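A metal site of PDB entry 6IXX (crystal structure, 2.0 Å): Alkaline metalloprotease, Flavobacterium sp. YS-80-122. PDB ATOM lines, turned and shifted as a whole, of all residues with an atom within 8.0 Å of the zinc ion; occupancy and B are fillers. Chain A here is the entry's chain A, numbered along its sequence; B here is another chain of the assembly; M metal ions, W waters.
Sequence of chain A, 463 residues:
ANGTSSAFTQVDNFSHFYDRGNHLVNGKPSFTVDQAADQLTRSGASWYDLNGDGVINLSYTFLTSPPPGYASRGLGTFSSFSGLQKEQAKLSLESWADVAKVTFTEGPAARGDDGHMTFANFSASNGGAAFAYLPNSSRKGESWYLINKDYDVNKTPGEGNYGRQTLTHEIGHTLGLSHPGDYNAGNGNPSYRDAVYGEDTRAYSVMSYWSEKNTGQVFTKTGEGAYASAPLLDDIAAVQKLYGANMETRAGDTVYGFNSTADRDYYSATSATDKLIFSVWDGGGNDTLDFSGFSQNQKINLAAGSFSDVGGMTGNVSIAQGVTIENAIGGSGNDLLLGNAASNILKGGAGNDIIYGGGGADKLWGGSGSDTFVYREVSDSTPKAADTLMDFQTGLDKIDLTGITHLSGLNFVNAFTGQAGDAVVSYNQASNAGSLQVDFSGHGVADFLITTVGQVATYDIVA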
ATOM      1  N   ALA A 130      -9.088  20.897 -17.947  1.00  0.00           N
ATOM      2  CA  ALA A 130      -9.814  22.153 -18.101  1.00  0.00           C
ATOM      3  C   ALA A 130      -9.063  22.980 -19.143  1.00  0.00           C
ATOM      4  O   ALA A 130      -7.907  22.691 -19.466  1.00  0.00           O
ATOM      5  CB  ALA A 130      -9.909  22.911 -16.777  1.00  0.00           C
ATOM      6  N   PHE A 131      -9.731  24.012 -19.663  1.00  0.00           N
ATOM      7  CA  PHE A 131      -9.104  24.929 -20.611  1.00  0.00           C
ATOM      8  C   PHE A 131      -9.855  26.258 -20.625  1.00  0.00           C
ATOM      9  O   PHE A 131     -10.996  26.363 -20.153  1.00  0.00           O
ATOM     10  CB  PHE A 131      -9.011  24.343 -22.029  1.00  0.00           C
ATOM     11  CG  PHE A 131     -10.349  24.124 -22.689  1.00  0.00           C
ATOM     12  CD1 PHE A 131     -11.055  22.954 -22.486  1.00  0.00           C
ATOM     13  CD2 PHE A 131     -10.896  25.091 -23.516  1.00  0.00           C
ATOM     14  CE1 PHE A 131     -12.282  22.752 -23.093  1.00  0.00           C
ATOM     15  CE2 PHE A 131     -12.121  24.898 -24.127  1.00  0.00           C
ATOM     16  CZ  PHE A 131     -12.822  23.723 -23.908  1.00  0.00           C
ATOM     17  N   ALA A 132      -9.192  27.270 -21.185  1.00  0.00           N
ATOM     18  CA  ALA A 132      -9.695  28.633 -21.201  1.00  0.00           C
ATOM     19  C   ALA A 132      -9.071  29.332 -22.393  1.00  0.00           C
ATOM     20  O   ALA A 132      -8.184  28.792 -23.065  1.00  0.00           O
ATOM     21  CB  ALA A 132      -9.376  29.373 -19.892  1.00  0.00           C
ATOM     22  N   TYR A 162      -6.664  20.372  -5.719  1.00  0.00           N
ATOM     23  CA  TYR A 162      -6.334  20.658  -7.110  1.00  0.00           C
ATOM     24  C   TYR A 162      -7.549  21.178  -7.872  1.00  0.00           C
ATOM     25  O   TYR A 162      -7.393  21.962  -8.820  1.00  0.00           O
ATOM     26  CB  TYR A 162      -5.756  19.403  -7.785  1.00  0.00           C
ATOM     27  CG  TYR A 162      -5.293  19.633  -9.217  1.00  0.00           C
ATOM     28  CD1 TYR A 162      -4.391  20.650  -9.532  1.00  0.00           C
ATOM     29  CD2 TYR A 162      -5.769  18.837 -10.255  1.00  0.00           C
ATOM     30  CE1 TYR A 162      -3.961  20.861 -10.833  1.00  0.00           C
ATOM     31  CE2 TYR A 162      -5.358  19.036 -11.566  1.00  0.00           C
ATOM     32  CZ  TYR A 162      -4.458  20.049 -11.844  1.00  0.00           C
ATOM     33  OH  TYR A 162      -4.059  20.240 -13.155  1.00  0.00           O
ATOM     34  N   THR A 166      -7.355  24.596  -9.976  1.00  0.00           N
ATOM     35  CA  THR A 166      -7.654  24.572 -11.401  1.00  0.00           C
ATOM     36  C   THR A 166      -8.554  25.738 -11.773  1.00  0.00           C
ATOM     37  O   THR A 166      -8.343  26.382 -12.816  1.00  0.00           O
ATOM     38  CB  THR A 166      -8.268  23.222 -11.789  1.00  0.00           C
ATOM     39  OG1 THR A 166      -7.283  22.178 -11.638  1.00  0.00           O
ATOM     40  CG2 THR A 166      -8.777  23.231 -13.239  1.00  0.00           C
ATOM     41  N   HIS A 169      -6.369  28.701 -11.810  1.00  0.00           N
ATOM     42  CA  HIS A 169      -5.457  28.604 -12.951  1.00  0.00           C
ATOM     43  C   HIS A 169      -6.156  29.000 -14.252  1.00  0.00           C
ATOM     44  O   HIS A 169      -5.655  29.853 -14.998  1.00  0.00           O
ATOM     45  CB  HIS A 169      -4.926  27.172 -13.018  1.00  0.00           C
ATOM     46  CG  HIS A 169      -4.121  26.846 -14.247  1.00  0.00           C
ATOM     47  ND1 HIS A 169      -2.773  26.525 -14.189  1.00  0.00           N
ATOM     48  CD2 HIS A 169      -4.468  26.758 -15.545  1.00  0.00           C
ATOM     49  CE1 HIS A 169      -2.332  26.270 -15.408  1.00  0.00           C
ATOM     50  NE2 HIS A 169      -3.339  26.400 -16.244  1.00  0.00           N
ATOM     51  N   GLU A 170      -7.311  28.390 -14.547  1.00  0.00           N
ATOM     52  CA  GLU A 170      -8.003  28.703 -15.801  1.00  0.00           C
ATOM     53  C   GLU A 170      -8.510  30.138 -15.812  1.00  0.00           C
ATOM     54  O   GLU A 170      -8.515  30.790 -16.868  1.00  0.00           O
ATOM     55  CB  GLU A 170      -9.152  27.713 -16.029  1.00  0.00           C
ATOM     56  CG  GLU A 170      -8.699  26.255 -16.194  1.00  0.00           C
ATOM     57  CD  GLU A 170      -7.721  26.024 -17.362  1.00  0.00           C
ATOM     58  OE1 GLU A 170      -7.682  26.863 -18.287  1.00  0.00           O
ATOM     59  OE2 GLU A 170      -6.983  25.016 -17.351  1.00  0.00           O
ATOM     60  N   ILE A 171      -8.939  30.667 -14.657  1.00  0.00           N
ATOM     61  CA  ILE A 171      -9.260  32.088 -14.590  1.00  0.00           C
ATOM     62  C   ILE A 171      -8.023  32.921 -14.931  1.00  0.00           C
ATOM     63  O   ILE A 171      -8.115  33.931 -15.644  1.00  0.00           O
ATOM     64  CB  ILE A 171      -9.836  32.448 -13.205  1.00  0.00           C
ATOM     65  CG1 ILE A 171     -11.214  31.814 -13.008  1.00  0.00           C
ATOM     66  CG2 ILE A 171      -9.947  33.964 -13.032  1.00  0.00           C
ATOM     67  CD1 ILE A 171     -11.780  32.038 -11.640  1.00  0.00           C
ATOM     68  N   GLY A 172      -6.852  32.491 -14.461  1.00  0.00           N
ATOM     69  CA  GLY A 172      -5.616  33.162 -14.831  1.00  0.00           C
ATOM     70  C   GLY A 172      -5.404  33.234 -16.332  1.00  0.00           C
ATOM     71  O   GLY A 172      -4.950  34.262 -16.859  1.00  0.00           O
ATOM     72  N   HIS A 173      -5.704  32.148 -17.040  1.00  0.00           N
ATOM     73  CA  HIS A 173      -5.663  32.191 -18.511  1.00  0.00           C
ATOM     74  C   HIS A 173      -6.595  33.277 -19.045  1.00  0.00           C
ATOM     75  O   HIS A 173      -6.176  34.136 -19.827  1.00  0.00           O
ATOM     76  CB  HIS A 173      -6.026  30.826 -19.095  1.00  0.00           C
ATOM     77  CG  HIS A 173      -4.917  29.810 -19.056  1.00  0.00           C
ATOM     78  ND1 HIS A 173      -3.612  30.116 -19.385  1.00  0.00           N
ATOM     79  CD2 HIS A 173      -4.923  28.496 -18.751  1.00  0.00           C
ATOM     80  CE1 HIS A 173      -2.864  29.030 -19.270  1.00  0.00           C
ATOM     81  NE2 HIS A 173      -3.637  28.033 -18.887  1.00  0.00           N
ATOM     82  N   LEU A 177      -2.675  35.333 -18.643  1.00  0.00           N
ATOM     83  CA  LEU A 177      -1.496  34.561 -18.265  1.00  0.00           C
ATOM     84  C   LEU A 177      -1.404  33.280 -19.084  1.00  0.00           C
ATOM     85  O   LEU A 177      -2.418  32.635 -19.371  1.00  0.00           O
ATOM     86  CB  LEU A 177      -1.538  34.221 -16.773  1.00  0.00           C
ATOM     87  CG  LEU A 177      -1.702  35.356 -15.752  1.00  0.00           C
ATOM     88  CD1 LEU A 177      -1.373  34.841 -14.364  1.00  0.00           C
ATOM     89  CD2 LEU A 177      -0.830  36.548 -16.101  1.00  0.00           C
ATOM     90  N   SER A 178      -0.176  32.921 -19.465  1.00  0.00           N
ATOM     91  CA  SER A 178       0.103  31.651 -20.103  1.00  0.00           C
ATOM     92  C   SER A 178       0.731  30.690 -19.096  1.00  0.00           C
ATOM     93  O   SER A 178       1.077  31.069 -17.980  1.00  0.00           O
ATOM     94  CB  SER A 178       1.036  31.840 -21.301  1.00  0.00           C
ATOM     95  OG  SER A 178       0.732  33.024 -22.010  1.00  0.00           O
ATOM     96  N   HIS A 179       0.858  29.441 -19.515  1.00  0.00           N
ATOM     97  CA  HIS A 179       1.763  28.559 -18.784  1.00  0.00           C
ATOM     98  C   HIS A 179       3.171  29.156 -18.826  1.00  0.00           C
ATOM     99  O   HIS A 179       3.534  29.808 -19.812  1.00  0.00           O
ATOM    100  CB  HIS A 179       1.772  27.163 -19.387  1.00  0.00           C
ATOM    101  CG  HIS A 179       0.455  26.456 -19.309  1.00  0.00           C
ATOM    102  ND1 HIS A 179       0.076  25.489 -20.219  1.00  0.00           N
ATOM    103  CD2 HIS A 179      -0.569  26.582 -18.434  1.00  0.00           C
ATOM    104  CE1 HIS A 179      -1.134  25.059 -19.904  1.00  0.00           C
ATOM    105  NE2 HIS A 179      -1.544  25.704 -18.831  1.00  0.00           N
ATOM    106  N   PRO A 180       3.966  28.968 -17.778  1.00  0.00           N
ATOM    107  CA  PRO A 180       5.347  29.491 -17.797  1.00  0.00           C
ATOM    108  C   PRO A 180       6.203  28.919 -18.915  1.00  0.00           C
ATOM    109  O   PRO A 180       7.255  29.494 -19.208  1.00  0.00           O
ATOM    110  CB  PRO A 180       5.894  29.095 -16.418  1.00  0.00           C
ATOM    111  CG  PRO A 180       4.659  28.932 -15.555  1.00  0.00           C
ATOM    112  CD  PRO A 180       3.613  28.374 -16.470  1.00  0.00           C
ATOM    113  N   TYR A 183       3.883  24.570 -23.239  1.00  0.00           N
ATOM    114  CA  TYR A 183       3.428  23.199 -23.074  1.00  0.00           C
ATOM    115  C   TYR A 183       1.950  23.188 -22.751  1.00  0.00           C
ATOM    116  O   TYR A 183       1.394  24.182 -22.278  1.00  0.00           O
ATOM    117  CB  TYR A 183       4.186  22.447 -21.961  1.00  0.00           C
ATOM    118  CG  TYR A 183       4.283  23.145 -20.603  1.00  0.00           C
ATOM    119  CD1 TYR A 183       3.179  23.237 -19.753  1.00  0.00           C
ATOM    120  CD2 TYR A 183       5.484  23.690 -20.179  1.00  0.00           C
ATOM    121  CE1 TYR A 183       3.283  23.868 -18.508  1.00  0.00           C
ATOM    122  CE2 TYR A 183       5.592  24.326 -18.946  1.00  0.00           C
ATOM    123  CZ  TYR A 183       4.504  24.402 -18.119  1.00  0.00           C
ATOM    124  OH  TYR A 183       4.633  25.017 -16.894  1.00  0.00           O
ATOM    125  N   ASN A 184       1.316  22.051 -22.991  1.00  0.00           N
ATOM    126  CA  ASN A 184      -0.118  21.919 -22.755  1.00  0.00           C
ATOM    127  C   ASN A 184      -0.467  20.454 -22.558  1.00  0.00           C
ATOM    128  O   ASN A 184       0.023  19.601 -23.300  1.00  0.00           O
ATOM    129  CB  ASN A 184      -0.929  22.493 -23.936  1.00  0.00           C
ATOM    130  CG  ASN A 184      -2.194  23.185 -23.476  1.00  0.00           C
ATOM    131  OD1 ASN A 184      -2.504  23.231 -22.285  1.00  0.00           O
ATOM    132  ND2 ASN A 184      -2.952  23.710 -24.442  1.00  0.00           N
ATOM    133  N   ALA A 185      -1.337  20.196 -21.587  1.00  0.00           N
ATOM    134  CA  ALA A 185      -1.806  18.839 -21.305  1.00  0.00           C
ATOM    135  C   ALA A 185      -2.450  18.223 -22.542  1.00  0.00           C
ATOM    136  O   ALA A 185      -3.268  18.860 -23.211  1.00  0.00           O
ATOM    137  CB  ALA A 185      -2.805  18.865 -20.148  1.00  0.00           C
ATOM    138  N   VAL A 206       0.563  29.342  -9.835  1.00  0.00           N
ATOM    139  CA  VAL A 206      -0.475  28.348 -10.080  1.00  0.00           C
ATOM    140  C   VAL A 206      -0.619  28.008 -11.551  1.00  0.00           C
ATOM    141  O   VAL A 206      -1.401  27.110 -11.900  1.00  0.00           O
ATOM    142  CB  VAL A 206      -1.839  28.826  -9.528  1.00  0.00           C
ATOM    143  CG1 VAL A 206      -1.739  29.184  -8.043  1.00  0.00           C
ATOM    144  CG2 VAL A 206      -2.364  30.010 -10.339  1.00  0.00           C
ATOM    145  N   MET A 207       0.116  28.699 -12.431  1.00  0.00           N
ATOM    146  CA  MET A 207       0.080  28.395 -13.860  1.00  0.00           C
ATOM    147  C   MET A 207       1.056  27.287 -14.236  1.00  0.00           C
ATOM    148  O   MET A 207       0.955  26.762 -15.351  1.00  0.00           O
ATOM    149  CB  MET A 207       0.383  29.639 -14.694  1.00  0.00           C
ATOM    150  CG  MET A 207      -0.448  30.860 -14.332  1.00  0.00           C
ATOM    151  SD  MET A 207      -2.209  30.528 -14.441  1.00  0.00           S
ATOM    152  CE  MET A 207      -2.316  30.028 -16.155  1.00  0.00           C
ATOM    153  N   SER A 208       1.992  26.944 -13.360  1.00  0.00           N
ATOM    154  CA  SER A 208       2.961  25.912 -13.650  1.00  0.00           C
ATOM    155  C   SER A 208       2.310  24.531 -13.668  1.00  0.00           C
ATOM    156  O   SER A 208       1.370  24.257 -12.916  1.00  0.00           O
ATOM    157  CB  SER A 208       4.074  25.924 -12.596  1.00  0.00           C
ATOM    158  OG  SER A 208       5.013  24.877 -12.863  1.00  0.00           O
ATOM    159  N   TYR A 209       2.838  23.643 -14.510  1.00  0.00           N
ATOM    160  CA  TYR A 209       2.473  22.223 -14.446  1.00  0.00           C
ATOM    161  C   TYR A 209       3.282  21.429 -13.415  1.00  0.00           C
ATOM    162  O   TYR A 209       2.890  20.301 -13.086  1.00  0.00           O
ATOM    163  CB  TYR A 209       2.677  21.564 -15.809  1.00  0.00           C
ATOM    164  CG  TYR A 209       1.509  21.720 -16.758  1.00  0.00           C
ATOM    165  CD1 TYR A 209       1.485  21.024 -17.948  1.00  0.00           C
ATOM    166  CD2 TYR A 209       0.448  22.556 -16.454  1.00  0.00           C
ATOM    167  CE1 TYR A 209       0.421  21.157 -18.836  1.00  0.00           C
ATOM    168  CE2 TYR A 209      -0.632  22.690 -17.323  1.00  0.00           C
ATOM    169  CZ  TYR A 209      -0.635  21.988 -18.515  1.00  0.00           C
ATOM    170  OH  TYR A 209      -1.704  22.103 -19.395  1.00  0.00           O
ATOM    171  N   SER B   1      -4.382  22.380 -18.178  1.00  0.00           N
ATOM    172  CA  SER B   1      -4.288  21.692 -16.882  1.00  0.00           C
ATOM    173  C   SER B   1      -4.153  20.173 -17.000  1.00  0.00           C
ATOM    174  O   SER B   1      -4.927  19.530 -17.673  1.00  0.00           O
ATOM    175  CB  SER B   1      -5.505  22.017 -15.989  1.00  0.00           C
ATOM    176  OG  SER B   1      -5.635  23.404 -15.739  1.00  0.00           O
ATOM    177  N   LEU B   2      -3.162  19.609 -16.316  1.00  0.00           N
ATOM    178  CA  LEU B   2      -2.995  18.166 -16.305  1.00  0.00           C
ATOM    179  C   LEU B   2      -4.150  17.490 -15.563  1.00  0.00           C
ATOM    180  O   LEU B   2      -4.707  18.032 -14.599  1.00  0.00           O
ATOM    181  CB  LEU B   2      -1.660  17.795 -15.663  1.00  0.00           C
ATOM    182  CG  LEU B   2      -0.442  18.329 -16.429  1.00  0.00           C
ATOM    183  CD1 LEU B   2       0.833  18.297 -15.566  1.00  0.00           C
ATOM    184  CD2 LEU B   2      -0.259  17.533 -17.710  1.00  0.00           C
HETATM  185 ZN    ZN M   1      -3.448  26.147 -18.256  1.00  0.00          ZN
HETATM  186  O   HOH W   1      -5.035  25.054 -19.074  1.00  0.00           O
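Water W1 lies within hydrogen-bond range of OE2 of Glu 170 and N of Ser 1 of chain B.
OE2 of Glu 170 touches the zinc ion, 3.8 Å away.
Ser 1 of chain B touches the zinc ion (N to ZN, 3.9 Å).
Of the 23 residues printed, 5 come within 4 Å of the zinc ion.
The nearest printed residue that does not touch the zinc ion is Tyr 209 (4.5 Å).
A ring nitrogen (ND1) of His 173 sits at hydrogen-bond distance from the backbone carbonyl oxygen (O) of Leu 177.
ND1 of His 169 lies within hydrogen-bond range of O of Val 206, at 2.7 Å.
ND1 of His 179 is in hydrogen-bond range of O of Tyr 183, at 2.8 Å.
The side-chain carboxylate (OE2) of Glu 170 lies within hydrogen-bond range of the side-chain hydroxyl (OG) of Ser 1 of chain B (2.6 Å).
The side-chain carboxylate (OE1) of Glu 170 lies within hydrogen-bond range of the backbone NH (N) of Ala 132.
OH of Tyr 209 lies within hydrogen-bond range of N of Ser 1 of chain B, at 3.0 Å.
The zinc ion is bound by NE2 of His 173, NE2 of His 169, NE2 of His 179 and water W1.
The zinc ion has four donor atoms within binding distance.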
